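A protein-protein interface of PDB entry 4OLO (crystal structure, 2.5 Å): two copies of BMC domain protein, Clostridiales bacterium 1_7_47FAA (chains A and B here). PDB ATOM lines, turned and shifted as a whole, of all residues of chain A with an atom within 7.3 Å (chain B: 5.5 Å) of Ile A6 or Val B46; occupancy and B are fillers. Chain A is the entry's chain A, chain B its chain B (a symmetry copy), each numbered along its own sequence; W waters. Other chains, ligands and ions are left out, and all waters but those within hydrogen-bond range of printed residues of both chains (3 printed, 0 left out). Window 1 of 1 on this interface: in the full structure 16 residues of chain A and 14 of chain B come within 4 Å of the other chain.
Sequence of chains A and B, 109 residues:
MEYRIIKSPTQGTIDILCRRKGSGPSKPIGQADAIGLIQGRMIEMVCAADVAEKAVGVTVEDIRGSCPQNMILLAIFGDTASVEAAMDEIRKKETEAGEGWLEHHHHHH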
ATOM      1  N   ARG A   4      12.793 -25.441 -21.274  1.00  0.00           N
ATOM      2  CA  ARG A   4      11.694 -25.966 -20.469  1.00  0.00           C
ATOM      3  C   ARG A   4      11.745 -25.356 -19.104  1.00  0.00           C
ATOM      4  O   ARG A   4      12.808 -24.997 -18.638  1.00  0.00           O
ATOM      5  CB  ARG A   4      11.741 -27.512 -20.336  1.00  0.00           C
ATOM      6  CG  ARG A   4      11.636 -28.305 -21.639  1.00  0.00           C
ATOM      7  CD  ARG A   4      10.264 -28.275 -22.289  1.00  0.00           C
ATOM      8  NE  ARG A   4       9.286 -29.093 -21.563  1.00  0.00           N
ATOM      9  CZ  ARG A   4       9.065 -30.386 -21.781  1.00  0.00           C
ATOM     10  NH1 ARG A   4       9.747 -31.036 -22.721  1.00  0.00           N
ATOM     11  NH2 ARG A   4       8.157 -31.038 -21.068  1.00  0.00           N
ATOM     12  N   ILE A   5      10.610 -25.296 -18.435  1.00  0.00           N
ATOM     13  CA  ILE A   5      10.498 -24.812 -17.073  1.00  0.00           C
ATOM     14  C   ILE A   5       9.705 -25.844 -16.239  1.00  0.00           C
ATOM     15  O   ILE A   5       8.712 -26.390 -16.708  1.00  0.00           O
ATOM     16  CB  ILE A   5       9.885 -23.370 -17.011  1.00  0.00           C
ATOM     17  CG1 ILE A   5      10.050 -22.757 -15.592  1.00  0.00           C
ATOM     18  CG2 ILE A   5       8.409 -23.339 -17.494  1.00  0.00           C
ATOM     19  CD1 ILE A   5       9.832 -21.261 -15.506  1.00  0.00           C
ATOM     20  N   ILE A   6      10.174 -26.118 -15.024  1.00  0.00           N
ATOM     21  CA  ILE A   6       9.522 -26.990 -14.057  1.00  0.00           C
ATOM     22  C   ILE A   6       9.123 -26.088 -12.892  1.00  0.00           C
ATOM     23  O   ILE A   6       9.986 -25.518 -12.218  1.00  0.00           O
ATOM     24  CB  ILE A   6      10.404 -28.186 -13.594  1.00  0.00           C
ATOM     25  CG1 ILE A   6      10.772 -29.133 -14.755  1.00  0.00           C
ATOM     26  CG2 ILE A   6       9.714 -28.943 -12.465  1.00  0.00           C
ATOM     27  CD1 ILE A   6      11.921 -30.105 -14.405  1.00  0.00           C
ATOM     28  N   LYS A   7       7.818 -25.961 -12.660  1.00  0.00           N
ATOM     29  CA  LYS A   7       7.271 -25.152 -11.557  1.00  0.00           C
ATOM     30  C   LYS A   7       7.033 -26.029 -10.338  1.00  0.00           C
ATOM     31  O   LYS A   7       6.498 -27.126 -10.463  1.00  0.00           O
ATOM     32  CB  LYS A   7       5.998 -24.382 -11.996  1.00  0.00           C
ATOM     33  CG  LYS A   7       6.344 -23.253 -12.982  1.00  0.00           C
ATOM     34  CD  LYS A   7       5.149 -22.644 -13.680  1.00  0.00           C
ATOM     35  CE  LYS A   7       5.606 -21.604 -14.680  1.00  0.00           C
ATOM     36  NZ  LYS A   7       4.525 -20.638 -15.018  1.00  0.00           N
ATOM     37  N   SER A   8       7.481 -25.564  -9.172  1.00  0.00           N
ATOM     38  CA  SER A   8       7.381 -26.262  -7.870  1.00  0.00           C
ATOM     39  C   SER A   8       8.006 -27.664  -7.968  1.00  0.00           C
ATOM     40  O   SER A   8       7.302 -28.662  -7.822  1.00  0.00           O
ATOM     41  CB  SER A   8       5.936 -26.312  -7.358  1.00  0.00           C
ATOM     42  OG  SER A   8       5.365 -25.016  -7.305  1.00  0.00           O
ATOM     43  N   PRO A   9       9.312 -27.769  -8.302  1.00  0.00           N
ATOM     44  CA  PRO A   9       9.910 -29.106  -8.458  1.00  0.00           C
ATOM     45  C   PRO A   9       9.927 -29.915  -7.171  1.00  0.00           C
ATOM     46  O   PRO A   9      10.026 -29.341  -6.094  1.00  0.00           O
ATOM     47  CB  PRO A   9      11.323 -28.792  -8.941  1.00  0.00           C
ATOM     48  CG  PRO A   9      11.606 -27.425  -8.379  1.00  0.00           C
ATOM     49  CD  PRO A   9      10.315 -26.710  -8.547  1.00  0.00           C
ATOM     50  N   THR A  10       9.833 -31.242  -7.281  1.00  0.00           N
ATOM     51  CA  THR A  10       9.918 -32.112  -6.102  1.00  0.00           C
ATOM     52  C   THR A  10      11.412 -32.258  -5.743  1.00  0.00           C
ATOM     53  O   THR A  10      12.283 -31.939  -6.557  1.00  0.00           O
ATOM     54  CB  THR A  10       9.268 -33.492  -6.381  1.00  0.00           C
ATOM     55  OG1 THR A  10      10.075 -34.222  -7.308  1.00  0.00           O
ATOM     56  CG2 THR A  10       7.896 -33.382  -6.944  1.00  0.00           C
ATOM     57  N   THR A  13      13.132 -34.630  -8.242  1.00  0.00           N
ATOM     58  CA  THR A  13      13.489 -33.953  -9.495  1.00  0.00           C
ATOM     59  C   THR A  13      14.824 -33.249  -9.296  1.00  0.00           C
ATOM     60  O   THR A  13      15.716 -33.363 -10.135  1.00  0.00           O
ATOM     61  CB  THR A  13      12.402 -32.938  -9.903  1.00  0.00           C
ATOM     62  OG1 THR A  13      11.143 -33.590  -9.895  1.00  0.00           O
ATOM     63  CG2 THR A  13      12.657 -32.320 -11.263  1.00  0.00           C
ATOM     64  N   ILE A  14      14.958 -32.533  -8.167  1.00  0.00           N
ATOM     65  CA  ILE A  14      16.193 -31.827  -7.840  1.00  0.00           C
ATOM     66  C   ILE A  14      17.342 -32.849  -7.678  1.00  0.00           C
ATOM     67  O   ILE A  14      18.411 -32.631  -8.237  1.00  0.00           O
ATOM     68  CB  ILE A  14      15.998 -30.837  -6.655  1.00  0.00           C
ATOM     69  CG1 ILE A  14      14.885 -29.816  -7.008  1.00  0.00           C
ATOM     70  CG2 ILE A  14      17.310 -30.114  -6.340  1.00  0.00           C
ATOM     71  CD1 ILE A  14      14.343 -28.991  -5.878  1.00  0.00           C
ATOM     72  N   ILE A  16      17.662 -35.798  -9.224  1.00  0.00           N
ATOM     73  CA  ILE A  16      18.017 -36.265 -10.574  1.00  0.00           C
ATOM     74  C   ILE A  16      18.997 -35.266 -11.207  1.00  0.00           C
ATOM     75  O   ILE A  16      20.025 -35.662 -11.741  1.00  0.00           O
ATOM     76  CB  ILE A  16      16.743 -36.502 -11.435  1.00  0.00           C
ATOM     77  CG1 ILE A  16      16.118 -37.857 -11.094  1.00  0.00           C
ATOM     78  CG2 ILE A  16      17.039 -36.411 -12.951  1.00  0.00           C
ATOM     79  CD1 ILE A  16      14.641 -37.906 -11.140  1.00  0.00           C
ATOM     80  N   LEU A  17      18.697 -33.971 -11.084  1.00  0.00           N
ATOM     81  CA  LEU A  17      19.536 -32.893 -11.588  1.00  0.00           C
ATOM     82  C   LEU A  17      20.887 -32.772 -10.864  1.00  0.00           C
ATOM     83  O   LEU A  17      21.919 -32.649 -11.519  1.00  0.00           O
ATOM     84  CB  LEU A  17      18.783 -31.548 -11.522  1.00  0.00           C
ATOM     85  CG  LEU A  17      17.805 -31.273 -12.623  1.00  0.00           C
ATOM     86  CD1 LEU A  17      17.031 -30.028 -12.323  1.00  0.00           C
ATOM     87  CD2 LEU A  17      18.503 -31.178 -13.978  1.00  0.00           C
ATOM     88  N   ASP A  33      11.565 -22.316  -6.233  1.00  0.00           N
ATOM     89  CA  ASP A  33      10.223 -22.701  -6.651  1.00  0.00           C
ATOM     90  C   ASP A  33       9.964 -22.881  -8.171  1.00  0.00           C
ATOM     91  O   ASP A  33       8.834 -23.180  -8.585  1.00  0.00           O
ATOM     92  CB  ASP A  33       9.116 -21.908  -5.900  1.00  0.00           C
ATOM     93  CG  ASP A  33       8.854 -20.452  -6.282  1.00  0.00           C
ATOM     94  OD1 ASP A  33       9.130 -20.080  -7.448  1.00  0.00           O
ATOM     95  OD2 ASP A  33       8.261 -19.712  -5.444  1.00  0.00           O
ATOM     96  N   ALA A  34      11.020 -22.732  -8.990  1.00  0.00           N
ATOM     97  CA  ALA A  34      11.005 -22.946 -10.434  1.00  0.00           C
ATOM     98  C   ALA A  34      12.412 -23.301 -10.914  1.00  0.00           C
ATOM     99  O   ALA A  34      13.382 -22.703 -10.442  1.00  0.00           O
ATOM    100  CB  ALA A  34      10.508 -21.707 -11.165  1.00  0.00           C
ATOM    101  N   ILE A  35      12.521 -24.274 -11.843  1.00  0.00           N
ATOM    102  CA  ILE A  35      13.777 -24.676 -12.495  1.00  0.00           C
ATOM    103  C   ILE A  35      13.589 -24.472 -13.997  1.00  0.00           C
ATOM    104  O   ILE A  35      12.672 -25.045 -14.585  1.00  0.00           O
ATOM    105  CB  ILE A  35      14.268 -26.132 -12.168  1.00  0.00           C
ATOM    106  CG1 ILE A  35      14.326 -26.389 -10.624  1.00  0.00           C
ATOM    107  CG2 ILE A  35      15.644 -26.397 -12.823  1.00  0.00           C
ATOM    108  CD1 ILE A  35      14.535 -27.848 -10.205  1.00  0.00           C
ATOM    109  N   GLY A  36      14.425 -23.626 -14.588  1.00  0.00           N
ATOM    110  CA  GLY A  36      14.445 -23.387 -16.021  1.00  0.00           C
ATOM    111  C   GLY A  36      15.529 -24.280 -16.568  1.00  0.00           C
ATOM    112  O   GLY A  36      16.635 -24.325 -16.014  1.00  0.00           O
ATOM    113  N   LEU A  37      15.215 -25.048 -17.605  1.00  0.00           N
ATOM    114  CA  LEU A  37      16.173 -25.972 -18.214  1.00  0.00           C
ATOM    115  C   LEU A  37      16.462 -25.569 -19.637  1.00  0.00           C
ATOM    116  O   LEU A  37      15.541 -25.217 -20.375  1.00  0.00           O
ATOM    117  CB  LEU A  37      15.650 -27.430 -18.179  1.00  0.00           C
ATOM    118  CG  LEU A  37      15.368 -28.073 -16.817  1.00  0.00           C
ATOM    119  CD1 LEU A  37      14.600 -29.348 -16.996  1.00  0.00           C
ATOM    120  CD2 LEU A  37      16.652 -28.294 -15.995  1.00  0.00           C
ATOM    121  N   GLN A  39      18.892 -26.928 -22.973  1.00  0.00           N
ATOM    122  CA  GLN A  39      19.740 -27.948 -23.566  1.00  0.00           C
ATOM    123  C   GLN A  39      20.133 -27.503 -24.963  1.00  0.00           C
ATOM    124  O   GLN A  39      19.286 -27.048 -25.729  1.00  0.00           O
ATOM    125  CB  GLN A  39      19.028 -29.301 -23.630  1.00  0.00           C
ATOM    126  CG  GLN A  39      19.999 -30.486 -23.817  1.00  0.00           C
ATOM    127  CD  GLN A  39      19.308 -31.826 -23.721  1.00  0.00           C
ATOM    128  OE1 GLN A  39      18.659 -32.147 -22.739  1.00  0.00           O
ATOM    129  NE2 GLN A  39      19.450 -32.660 -24.725  1.00  0.00           N
ATOM    130  N   ILE A  63      24.796 -29.045 -15.591  1.00  0.00           N
ATOM    131  CA  ILE A  63      24.523 -30.455 -15.315  1.00  0.00           C
ATOM    132  C   ILE A  63      25.482 -31.281 -16.168  1.00  0.00           C
ATOM    133  O   ILE A  63      25.432 -31.209 -17.399  1.00  0.00           O
ATOM    134  CB  ILE A  63      23.007 -30.786 -15.508  1.00  0.00           C
ATOM    135  CG1 ILE A  63      22.063 -29.767 -14.789  1.00  0.00           C
ATOM    136  CG2 ILE A  63      22.690 -32.230 -15.182  1.00  0.00           C
ATOM    137  CD1 ILE A  63      22.290 -29.502 -13.260  1.00  0.00           C
ATOM    138  N   LEU A  73      23.400 -30.281 -19.688  1.00  0.00           N
ATOM    139  CA  LEU A  73      22.232 -29.397 -19.556  1.00  0.00           C
ATOM    140  C   LEU A  73      22.539 -28.197 -18.649  1.00  0.00           C
ATOM    141  O   LEU A  73      23.450 -28.259 -17.813  1.00  0.00           O
ATOM    142  CB  LEU A  73      21.125 -30.295 -18.936  1.00  0.00           C
ATOM    143  CG  LEU A  73      19.709 -29.827 -18.654  1.00  0.00           C
ATOM    144  CD1 LEU A  73      18.973 -29.460 -19.923  1.00  0.00           C
ATOM    145  CD2 LEU A  73      18.926 -30.952 -17.988  1.00  0.00           C
ATOM    146  N   ILE A  76      18.608 -23.525 -14.140  1.00  0.00           N
ATOM    147  CA  ILE A  76      18.460 -22.166 -13.598  1.00  0.00           C
ATOM    148  C   ILE A  76      17.414 -22.214 -12.509  1.00  0.00           C
ATOM    149  O   ILE A  76      16.257 -22.503 -12.780  1.00  0.00           O
ATOM    150  CB  ILE A  76      18.104 -21.217 -14.788  1.00  0.00           C
ATOM    151  CG1 ILE A  76      19.337 -20.929 -15.622  1.00  0.00           C
ATOM    152  CG2 ILE A  76      17.426 -19.921 -14.413  1.00  0.00           C
ATOM    153  CD1 ILE A  76      18.976 -20.796 -17.039  1.00  0.00           C
ATOM    154  N   GLY A  78      15.352 -20.534  -9.114  1.00  0.00           N
ATOM    155  CA  GLY A  78      14.855 -19.317  -8.487  1.00  0.00           C
ATOM    156  C   GLY A  78      13.348 -19.246  -8.479  1.00  0.00           C
ATOM    157  O   GLY A  78      12.669 -20.239  -8.743  1.00  0.00           O
ATOM    158  N   THR A  80       9.744 -18.143 -10.007  1.00  0.00           N
ATOM    159  CA  THR A  80       9.204 -18.200 -11.365  1.00  0.00           C
ATOM    160  C   THR A  80       9.515 -16.957 -12.208  1.00  0.00           C
ATOM    161  O   THR A  80      10.027 -17.096 -13.318  1.00  0.00           O
ATOM    162  CB  THR A  80       7.709 -18.512 -11.323  1.00  0.00           C
ATOM    163  OG1 THR A  80       7.512 -19.681 -10.533  1.00  0.00           O
ATOM    164  CG2 THR A  80       7.114 -18.720 -12.715  1.00  0.00           C
ATOM    165  N   VAL A  83      13.258 -16.728 -13.062  1.00  0.00           N
ATOM    166  CA  VAL A  83      13.600 -17.835 -13.964  1.00  0.00           C
ATOM    167  C   VAL A  83      13.081 -17.514 -15.378  1.00  0.00           C
ATOM    168  O   VAL A  83      13.858 -17.554 -16.327  1.00  0.00           O
ATOM    169  CB  VAL A  83      13.139 -19.217 -13.413  1.00  0.00           C
ATOM    170  CG1 VAL A  83      13.239 -20.305 -14.477  1.00  0.00           C
ATOM    171  CG2 VAL A  83      13.960 -19.609 -12.191  1.00  0.00           C
ATOM    172  N   ARG B  41      15.262 -37.135 -24.676  1.00  0.00           N
ATOM    173  CA  ARG B  41      16.349 -36.219 -24.412  1.00  0.00           C
ATOM    174  C   ARG B  41      16.317 -35.898 -22.920  1.00  0.00           C
ATOM    175  O   ARG B  41      15.237 -35.962 -22.296  1.00  0.00           O
ATOM    176  CB  ARG B  41      16.183 -34.972 -25.271  1.00  0.00           C
ATOM    177  CG  ARG B  41      16.541 -35.225 -26.740  1.00  0.00           C
ATOM    178  CD  ARG B  41      16.353 -34.024 -27.647  1.00  0.00           C
ATOM    179  NE  ARG B  41      15.045 -33.376 -27.478  1.00  0.00           N
ATOM    180  CZ  ARG B  41      13.955 -33.637 -28.198  1.00  0.00           C
ATOM    181  NH1 ARG B  41      13.985 -34.561 -29.153  1.00  0.00           N
ATOM    182  NH2 ARG B  41      12.826 -32.980 -27.963  1.00  0.00           N
ATOM    183  N   MET B  42      17.484 -35.609 -22.323  1.00  0.00           N
ATOM    184  CA  MET B  42      17.519 -35.364 -20.886  1.00  0.00           C
ATOM    185  C   MET B  42      16.544 -34.320 -20.369  1.00  0.00           C
ATOM    186  O   MET B  42      15.888 -34.565 -19.357  1.00  0.00           O
ATOM    187  CB  MET B  42      18.929 -35.144 -20.348  1.00  0.00           C
ATOM    188  CG  MET B  42      19.048 -35.595 -18.910  1.00  0.00           C
ATOM    189  SD  MET B  42      20.470 -34.843 -18.112  1.00  0.00           S
ATOM    190  CE  MET B  42      21.662 -36.236 -18.129  1.00  0.00           C
ATOM    191  N   ILE B  43      16.429 -33.178 -21.068  1.00  0.00           N
ATOM    192  CA  ILE B  43      15.523 -32.091 -20.679  1.00  0.00           C
ATOM    193  C   ILE B  43      14.069 -32.605 -20.566  1.00  0.00           C
ATOM    194  O   ILE B  43      13.406 -32.325 -19.585  1.00  0.00           O
ATOM    195  CB  ILE B  43      15.719 -30.865 -21.625  1.00  0.00           C
ATOM    196  CG1 ILE B  43      15.038 -29.602 -21.087  1.00  0.00           C
ATOM    197  CG2 ILE B  43      15.343 -31.184 -23.087  1.00  0.00           C
ATOM    198  CD1 ILE B  43      15.502 -28.349 -21.680  1.00  0.00           C
ATOM    199  N   GLU B  44      13.624 -33.418 -21.540  1.00  0.00           N
ATOM    200  CA  GLU B  44      12.293 -34.023 -21.600  1.00  0.00           C
ATOM    201  C   GLU B  44      12.087 -34.995 -20.431  1.00  0.00           C
ATOM    202  O   GLU B  44      11.008 -35.004 -19.821  1.00  0.00           O
ATOM    203  CB  GLU B  44      12.117 -34.811 -22.907  1.00  0.00           C
ATOM    204  CG  GLU B  44      12.576 -34.124 -24.167  1.00  0.00           C
ATOM    205  CD  GLU B  44      12.197 -34.918 -25.393  1.00  0.00           C
ATOM    206  OE1 GLU B  44      12.864 -35.928 -25.712  1.00  0.00           O
ATOM    207  OE2 GLU B  44      11.204 -34.522 -26.035  1.00  0.00           O
ATOM    208  N   MET B  45      13.114 -35.850 -20.155  1.00  0.00           N
ATOM    209  CA  MET B  45      13.129 -36.848 -19.084  1.00  0.00           C
ATOM    210  C   MET B  45      13.070 -36.220 -17.678  1.00  0.00           C
ATOM    211  O   MET B  45      12.378 -36.776 -16.818  1.00  0.00           O
ATOM    212  CB  MET B  45      14.326 -37.816 -19.212  1.00  0.00           C
ATOM    213  CG  MET B  45      14.158 -38.884 -20.310  1.00  0.00           C
ATOM    214  SD  MET B  45      15.402 -40.235 -20.403  1.00  0.00           S
ATOM    215  CE  MET B  45      16.976 -39.309 -20.483  1.00  0.00           C
ATOM    216  N   VAL B  46      13.780 -35.078 -17.444  1.00  0.00           N
ATOM    217  CA  VAL B  46      13.798 -34.366 -16.153  1.00  0.00           C
ATOM    218  C   VAL B  46      12.382 -33.806 -15.898  1.00  0.00           C
ATOM    219  O   VAL B  46      11.876 -33.921 -14.780  1.00  0.00           O
ATOM    220  CB  VAL B  46      14.921 -33.279 -16.050  1.00  0.00           C
ATOM    221  CG1 VAL B  46      14.798 -32.469 -14.767  1.00  0.00           C
ATOM    222  CG2 VAL B  46      16.306 -33.904 -16.138  1.00  0.00           C
ATOM    223  N   CYS B  47      11.721 -33.299 -16.961  1.00  0.00           N
ATOM    224  CA  CYS B  47      10.352 -32.792 -16.898  1.00  0.00           C
ATOM    225  C   CYS B  47       9.372 -33.906 -16.561  1.00  0.00           C
ATOM    226  O   CYS B  47       8.516 -33.727 -15.688  1.00  0.00           O
ATOM    227  CB  CYS B  47       9.976 -32.089 -18.198  1.00  0.00           C
ATOM    228  SG  CYS B  47      10.813 -30.510 -18.424  1.00  0.00           S
ATOM    229  N   ALA B  48       9.515 -35.056 -17.253  1.00  0.00           N
ATOM    230  CA  ALA B  48       8.716 -36.270 -17.071  1.00  0.00           C
ATOM    231  C   ALA B  48       8.881 -36.801 -15.634  1.00  0.00           C
ATOM    232  O   ALA B  48       7.881 -37.164 -14.994  1.00  0.00           O
ATOM    233  CB  ALA B  48       9.147 -37.335 -18.092  1.00  0.00           C
ATOM    234  N   ALA B  49      10.143 -36.818 -15.127  1.00  0.00           N
ATOM    235  CA  ALA B  49      10.493 -37.273 -13.766  1.00  0.00           C
ATOM    236  C   ALA B  49       9.708 -36.488 -12.753  1.00  0.00           C
ATOM    237  O   ALA B  49       9.217 -37.085 -11.804  1.00  0.00           O
ATOM    238  CB  ALA B  49      11.990 -37.117 -13.510  1.00  0.00           C
ATOM    239  N   ASP B  50       9.534 -35.160 -12.975  1.00  0.00           N
ATOM    240  CA  ASP B  50       8.773 -34.317 -12.051  1.00  0.00           C
ATOM    241  C   ASP B  50       7.298 -34.690 -11.981  1.00  0.00           C
ATOM    242  O   ASP B  50       6.736 -34.718 -10.893  1.00  0.00           O
ATOM    243  CB  ASP B  50       8.962 -32.826 -12.348  1.00  0.00           C
ATOM    244  CG  ASP B  50       8.481 -31.952 -11.204  1.00  0.00           C
ATOM    245  OD1 ASP B  50       9.111 -31.992 -10.124  1.00  0.00           O
ATOM    246  OD2 ASP B  50       7.472 -31.230 -11.390  1.00  0.00           O
ATOM    247  N   LYS B  54       5.245 -36.516  -8.679  1.00  0.00           N
ATOM    248  CA  LYS B  54       3.996 -35.927  -8.177  1.00  0.00           C
ATOM    249  C   LYS B  54       2.819 -36.905  -8.346  1.00  0.00           C
ATOM    250  O   LYS B  54       1.729 -36.638  -7.864  1.00  0.00           O
ATOM    251  CB  LYS B  54       3.721 -34.588  -8.880  1.00  0.00           C
ATOM    252  CG  LYS B  54       4.658 -33.485  -8.417  1.00  0.00           C
ATOM    253  CD  LYS B  54       4.610 -32.261  -9.312  1.00  0.00           C
ATOM    254  CE  LYS B  54       5.440 -31.157  -8.702  1.00  0.00           C
ATOM    255  NZ  LYS B  54       5.520 -29.975  -9.591  1.00  0.00           N
ATOM    256  N   MET B  71      22.011 -39.828 -17.555  1.00  0.00           N
ATOM    257  CA  MET B  71      20.652 -40.376 -17.534  1.00  0.00           C
ATOM    258  C   MET B  71      20.225 -40.818 -18.931  1.00  0.00           C
ATOM    259  O   MET B  71      20.157 -39.992 -19.851  1.00  0.00           O
ATOM    260  CB  MET B  71      19.656 -39.361 -16.951  1.00  0.00           C
ATOM    261  CG  MET B  71      18.261 -39.908 -16.807  1.00  0.00           C
ATOM    262  SD  MET B  71      17.078 -38.674 -16.225  1.00  0.00           S
ATOM    263  CE  MET B  71      15.610 -39.655 -16.204  1.00  0.00           C
HETATM  264  O   HOH W   1      20.173 -35.913 -24.067  1.00  0.00           O
HETATM  265  O   HOH W   2       8.532 -34.476 -20.620  1.00  0.00           O
HETATM  266  O   HOH W   3       7.729 -28.985 -17.309  1.00  0.00           O
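Printed residues of chain A that touch a printed residue of chain B: Arg A4, Ile A6, Lys A7, Ser A8, Pro A9, Thr A10, Thr A13, Ile A16, Leu A17, Leu A37, Gln A39 and Leu A73.
Of the 12 printed residues of chain B, 8 touch a printed residue of chain A.
Hydrophobic or aromatic side chains of chain B that line the printed part of chain A: Met B42, Ile B43, Val B46, Ala B49 and Met B71.
Among the printed residues, 20 pairs touch across the chains.
Among the printed residues, no Asp or Glu carboxylate lies within 4 Å of a Lys or Arg side-chain nitrogen of the other chain.
No position is printed for both chains.
Water W2 bridges the backbone carbonyl oxygen of Glu B44 and the guanidinium group of Arg A4.
Water W3 bridges the backbone carbonyl oxygen (O) of Ile A5 (2.8 Å) and the side-chain sulfur (SG) of Cys B47 (3.6 Å).
Water W1 lies within hydrogen-bond range of the backbone NH of Met B42 (3.2 Å) and the side-chain amide nitrogen of Gln A39 (3.4 Å).
Printed residues of chain B within 4 Å of Ile A6: Val B46, Cys B47 and Asp B50.
Of the printed residues of chain B, Thr A10 touches Asp B50 (3.0 Å) and Lys B54 (3.6 Å).
Arg B41 touches none of the printed residues of chain A.
Val B46 touches just these residues of chain A: Ile A6 (3.7 Å), Thr A13 (3.9 Å), Leu A17 (3.9 Å) and Leu A37 (3.8 Å).
Printed residues of chain A within 4 Å of Cys B47: Arg A4 and Ile A6.
Of the printed residues of chain A, Ala B49 touches Ile A16 (3.6 Å).
The nearest residue of chain B that does not touch Ile A6 is Lys B54 (5.2 Å).
The backbone carbonyl oxygen of Arg A4 is in hydrogen-bond range of the backbone NH of Leu A37 (2.6 Å).
The backbone carbonyl oxygen (O) of Asp A33 lies within hydrogen-bond range of the backbone NH (N) of Ser A8 (2.8 Å).
OG1 of Thr A13 sits at hydrogen-bond distance from OG1 of Thr A10.
N of Ile A63 lies within hydrogen-bond range of O of Leu A73.
The backbone carbonyl oxygen (O) of Ile B43 is in hydrogen-bond range of the side-chain sulfur (SG) of Cys B47 (3.4 Å).
The side-chain carboxylate of Asp B50 lies within salt-bridge range of the side-chain amino group of Lys B54 (2.9 Å).
Arg A4 touches Ile B43.
Ile A6 touches Cys B47.
CG2 of Ile A6 touches OD2 of Asp B50, 3.4 Å away.
Pro A9 touches Asp B50.
Thr A10 touches Lys B54 (CG2 to CG, 3.6 Å).
Ile A16 touches Ala B49 (CD1 to CB, 3.6 Å).
CD1 of Ile B43 touches O of Leu A37, at 3.4 Å.
CG1 of Val B46 touches CD1 of Leu A37, 3.8 Å away.
Gln A39 touches Met B42 (OE1 to N, 3.7 Å).
Leu A73 touches Ile B43.
NE of Arg A4 sits close to SG of Cys B47, at 3.8 Å.
The backbone carbonyl oxygen of Lys A7 sits at hydrogen-bond distance from the side-chain amino group of Lys B54 (3.1 Å).
The backbone carbonyl oxygen (O) of Ser A8 lies within hydrogen-bond range of the side-chain amino group (NZ) of Lys B54.
N of Thr A10 lies within hydrogen-bond range of OD1 of Asp B50, at 3.0 Å.
The side-chain carboxylate (OD1) of Asp B50 sits at hydrogen-bond distance from the side-chain hydroxyl (OG1) of Thr A13 (2.6 Å).
OE1 of Gln A39 is in hydrogen-bond range of N of Ile B43 (3.0 Å).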
